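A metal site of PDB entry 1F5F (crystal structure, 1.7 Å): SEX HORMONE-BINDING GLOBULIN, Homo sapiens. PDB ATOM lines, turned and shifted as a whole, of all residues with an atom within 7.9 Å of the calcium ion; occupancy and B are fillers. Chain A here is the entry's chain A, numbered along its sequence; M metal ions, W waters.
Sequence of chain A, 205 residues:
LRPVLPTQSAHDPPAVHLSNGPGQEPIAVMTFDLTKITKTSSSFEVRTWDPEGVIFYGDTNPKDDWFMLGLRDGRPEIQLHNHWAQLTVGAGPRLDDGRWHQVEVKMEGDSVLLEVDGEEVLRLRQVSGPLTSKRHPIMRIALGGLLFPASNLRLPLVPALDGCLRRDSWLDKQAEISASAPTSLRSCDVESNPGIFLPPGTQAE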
ATOM      1  N   SER A  19      18.319  25.637  -8.272  1.00  0.00           N
ATOM      2  CA  SER A  19      18.211  25.927  -6.831  1.00  0.00           C
ATOM      3  C   SER A  19      18.367  27.404  -6.519  1.00  0.00           C
ATOM      4  O   SER A  19      19.485  27.882  -6.773  1.00  0.00           O
ATOM      5  CB  SER A  19      19.247  25.073  -6.095  1.00  0.00           C
ATOM      6  OG  SER A  19      19.831  25.701  -4.978  1.00  0.00           O
ATOM      7  N   THR A  48      25.218  19.656 -14.379  1.00  0.00           N
ATOM      8  CA  THR A  48      25.611  20.008 -13.028  1.00  0.00           C
ATOM      9  C   THR A  48      27.067  19.559 -12.778  1.00  0.00           C
ATOM     10  O   THR A  48      27.551  18.638 -13.427  1.00  0.00           O
ATOM     11  CB  THR A  48      24.698  19.360 -11.981  1.00  0.00           C
ATOM     12  OG1 THR A  48      24.887  19.804 -10.646  1.00  0.00           O
ATOM     13  CG2 THR A  48      24.792  17.871 -12.108  1.00  0.00           C
ATOM     14  N   TRP A  49      27.636  20.156 -11.762  1.00  0.00           N
ATOM     15  CA  TRP A  49      28.909  19.757 -11.172  1.00  0.00           C
ATOM     16  C   TRP A  49      28.652  19.262  -9.759  1.00  0.00           C
ATOM     17  O   TRP A  49      29.605  18.823  -9.105  1.00  0.00           O
ATOM     18  CB  TRP A  49      29.851  20.993 -11.012  1.00  0.00           C
ATOM     19  CG  TRP A  49      30.329  21.435 -12.369  1.00  0.00           C
ATOM     20  CD1 TRP A  49      29.890  22.506 -13.084  1.00  0.00           C
ATOM     21  CD2 TRP A  49      31.278  20.757 -13.213  1.00  0.00           C
ATOM     22  NE1 TRP A  49      30.521  22.558 -14.305  1.00  0.00           N
ATOM     23  CE2 TRP A  49      31.370  21.494 -14.407  1.00  0.00           C
ATOM     24  CE3 TRP A  49      32.050  19.606 -13.054  1.00  0.00           C
ATOM     25  CZ2 TRP A  49      32.222  21.110 -15.445  1.00  0.00           C
ATOM     26  CZ3 TRP A  49      32.894  19.230 -14.083  1.00  0.00           C
ATOM     27  CH2 TRP A  49      32.963  19.983 -15.267  1.00  0.00           C
ATOM     28  N   ASP A  50      27.408  19.306  -9.286  1.00  0.00           N
ATOM     29  CA  ASP A  50      27.070  19.034  -7.884  1.00  0.00           C
ATOM     30  C   ASP A  50      26.808  17.534  -7.742  1.00  0.00           C
ATOM     31  O   ASP A  50      26.008  17.024  -8.530  1.00  0.00           O
ATOM     32  CB  ASP A  50      25.776  19.772  -7.471  1.00  0.00           C
ATOM     33  CG  ASP A  50      25.426  19.797  -6.014  1.00  0.00           C
ATOM     34  OD1 ASP A  50      26.025  19.045  -5.196  1.00  0.00           O
ATOM     35  OD2 ASP A  50      24.546  20.522  -5.449  1.00  0.00           O
ATOM     36  N   PRO A  51      27.572  16.820  -6.933  1.00  0.00           N
ATOM     37  CA  PRO A  51      27.294  15.408  -6.701  1.00  0.00           C
ATOM     38  C   PRO A  51      26.046  15.020  -5.955  1.00  0.00           C
ATOM     39  O   PRO A  51      25.739  13.817  -5.961  1.00  0.00           O
ATOM     40  CB  PRO A  51      28.547  14.941  -5.917  1.00  0.00           C
ATOM     41  CG  PRO A  51      28.865  16.152  -5.076  1.00  0.00           C
ATOM     42  CD  PRO A  51      28.539  17.360  -5.926  1.00  0.00           C
ATOM     43  N   GLU A  52      25.315  15.878  -5.280  1.00  0.00           N
ATOM     44  CA  GLU A  52      24.250  15.479  -4.378  1.00  0.00           C
ATOM     45  C   GLU A  52      23.156  16.559  -4.470  1.00  0.00           C
ATOM     46  O   GLU A  52      23.474  17.749  -4.431  1.00  0.00           O
ATOM     47  CB  GLU A  52      24.686  15.356  -2.927  1.00  0.00           C
ATOM     48  CG  GLU A  52      23.660  14.890  -1.930  1.00  0.00           C
ATOM     49  CD  GLU A  52      24.187  14.497  -0.566  1.00  0.00           C
ATOM     50  OE1 GLU A  52      25.133  13.665  -0.442  1.00  0.00           O
ATOM     51  OE2 GLU A  52      23.565  14.913   0.436  1.00  0.00           O
ATOM     52  N   GLY A  53      21.912  16.136  -4.500  1.00  0.00           N
ATOM     53  CA  GLY A  53      20.804  17.093  -4.447  1.00  0.00           C
ATOM     54  C   GLY A  53      19.525  16.376  -4.936  1.00  0.00           C
ATOM     55  O   GLY A  53      19.616  15.378  -5.649  1.00  0.00           O
ATOM     56  N   VAL A  54      18.423  17.129  -4.879  1.00  0.00           N
ATOM     57  CA  VAL A  54      17.158  16.640  -5.457  1.00  0.00           C
ATOM     58  C   VAL A  54      17.052  17.150  -6.882  1.00  0.00           C
ATOM     59  O   VAL A  54      17.030  18.401  -6.960  1.00  0.00           O
ATOM     60  CB  VAL A  54      15.942  17.130  -4.678  1.00  0.00           C
ATOM     61  CG1 VAL A  54      14.610  16.662  -5.349  1.00  0.00           C
ATOM     62  CG2 VAL A  54      15.933  16.573  -3.270  1.00  0.00           C
ATOM     63  N   LEU A  71      20.573  13.144  -7.184  1.00  0.00           N
ATOM     64  CA  LEU A  71      21.939  12.656  -7.225  1.00  0.00           C
ATOM     65  C   LEU A  71      22.510  12.490  -5.818  1.00  0.00           C
ATOM     66  O   LEU A  71      22.251  13.062  -4.783  1.00  0.00           O
ATOM     67  CB  LEU A  71      22.866  13.626  -7.972  1.00  0.00           C
ATOM     68  CG  LEU A  71      22.475  13.901  -9.438  1.00  0.00           C
ATOM     69  CD1 LEU A  71      23.575  14.789 -10.043  1.00  0.00           C
ATOM     70  CD2 LEU A  71      22.331  12.662 -10.324  1.00  0.00           C
ATOM     71  N   VAL A 158      21.234  16.357   1.367  1.00  0.00           N
ATOM     72  CA  VAL A 158      21.063  17.830   1.369  1.00  0.00           C
ATOM     73  C   VAL A 158      20.500  18.129  -0.023  1.00  0.00           C
ATOM     74  O   VAL A 158      21.147  17.943  -1.037  1.00  0.00           O
ATOM     75  CB  VAL A 158      22.440  18.481   1.614  1.00  0.00           C
ATOM     76  CG1 VAL A 158      22.293  20.010   1.450  1.00  0.00           C
ATOM     77  CG2 VAL A 158      22.885  18.122   3.009  1.00  0.00           C
ATOM     78  N   PRO A 159      19.253  18.654  -0.045  1.00  0.00           N
ATOM     79  CA  PRO A 159      18.466  18.812  -1.250  1.00  0.00           C
ATOM     80  C   PRO A 159      18.957  19.749  -2.303  1.00  0.00           C
ATOM     81  O   PRO A 159      18.741  19.590  -3.503  1.00  0.00           O
ATOM     82  CB  PRO A 159      17.030  19.134  -0.802  1.00  0.00           C
ATOM     83  CG  PRO A 159      17.165  19.507   0.629  1.00  0.00           C
ATOM     84  CD  PRO A 159      18.447  18.912   1.161  1.00  0.00           C
ATOM     85  N   ALA A 160      19.711  20.795  -1.857  1.00  0.00           N
ATOM     86  CA  ALA A 160      20.166  21.742  -2.870  1.00  0.00           C
ATOM     87  C   ALA A 160      21.020  21.085  -3.925  1.00  0.00           C
ATOM     88  O   ALA A 160      22.093  20.493  -3.762  1.00  0.00           O
ATOM     89  CB  ALA A 160      20.909  22.916  -2.238  1.00  0.00           C
ATOM     90  N   LEU A 161      20.589  21.211  -5.155  1.00  0.00           N
ATOM     91  CA  LEU A 161      21.269  20.802  -6.375  1.00  0.00           C
ATOM     92  C   LEU A 161      21.569  22.040  -7.228  1.00  0.00           C
ATOM     93  O   LEU A 161      20.722  22.547  -7.961  1.00  0.00           O
ATOM     94  CB  LEU A 161      20.493  19.799  -7.192  1.00  0.00           C
ATOM     95  CG  LEU A 161      21.200  19.123  -8.366  1.00  0.00           C
ATOM     96  CD1 LEU A 161      22.432  18.368  -7.920  1.00  0.00           C
ATOM     97  CD2 LEU A 161      20.191  18.187  -9.043  1.00  0.00           C
ATOM     98  N   ASP A 162      22.838  22.433  -7.254  1.00  0.00           N
ATOM     99  CA  ASP A 162      23.274  23.478  -8.175  1.00  0.00           C
ATOM    100  C   ASP A 162      23.516  22.969  -9.573  1.00  0.00           C
ATOM    101  O   ASP A 162      24.585  22.498  -9.974  1.00  0.00           O
ATOM    102  CB  ASP A 162      24.527  24.143  -7.548  1.00  0.00           C
ATOM    103  CG  ASP A 162      24.143  24.682  -6.172  1.00  0.00           C
ATOM    104  OD1 ASP A 162      23.230  25.549  -6.123  1.00  0.00           O
ATOM    105  OD2 ASP A 162      24.689  24.233  -5.145  1.00  0.00           O
ATOM    106  N   GLY A 163      22.503  23.047 -10.441  1.00  0.00           N
ATOM    107  CA  GLY A 163      22.588  22.589 -11.799  1.00  0.00           C
ATOM    108  C   GLY A 163      21.528  23.290 -12.650  1.00  0.00           C
ATOM    109  O   GLY A 163      20.717  24.054 -12.136  1.00  0.00           O
HETATM  110 CA    CA M   1      24.240  19.842  -3.696  1.00  0.00          CA
HETATM  111  O   HOH W   1      23.693  19.207  -1.870  1.00  0.00           O
HETATM  112  O   HOH W   2      26.335  19.349  -2.595  1.00  0.00           O
HETATM  113  O   HOH W   3      24.923  21.920  -2.942  1.00  0.00           O
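The side-chain carboxylate of Asp 50 sits close to the backbone NH of Asp 162.
N of Asp 50 sits at hydrogen-bond distance from OG1 of Thr 48, at 2.9 Å.
The side-chain carboxylate of Glu 52 is in hydrogen-bond range of the backbone NH of Val 158 (2.9 Å).
Of the 15 residues printed, 3 come within 4 Å of the calcium ion.
The nearest printed residue that does not touch the calcium ion is Leu 161 (4.1 Å).
OD2 of Asp 50 binds the calcium ion (1.9 Å).
Water W1 binds the calcium ion, 2.0 Å away.
O of Ala 160 is bound to the calcium ion.
Water W3 binds the calcium ion, 2.3 Å away.
The calcium ion is bound by O of Glu 52 (2.3 Å).
Water W2 is bound to the calcium ion (2.4 Å).
The calcium ion is bound by the side-chain carboxylate (OD1) of Asp 50 (2.5 Å).
The calcium ion has seven donor atoms within binding distance.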
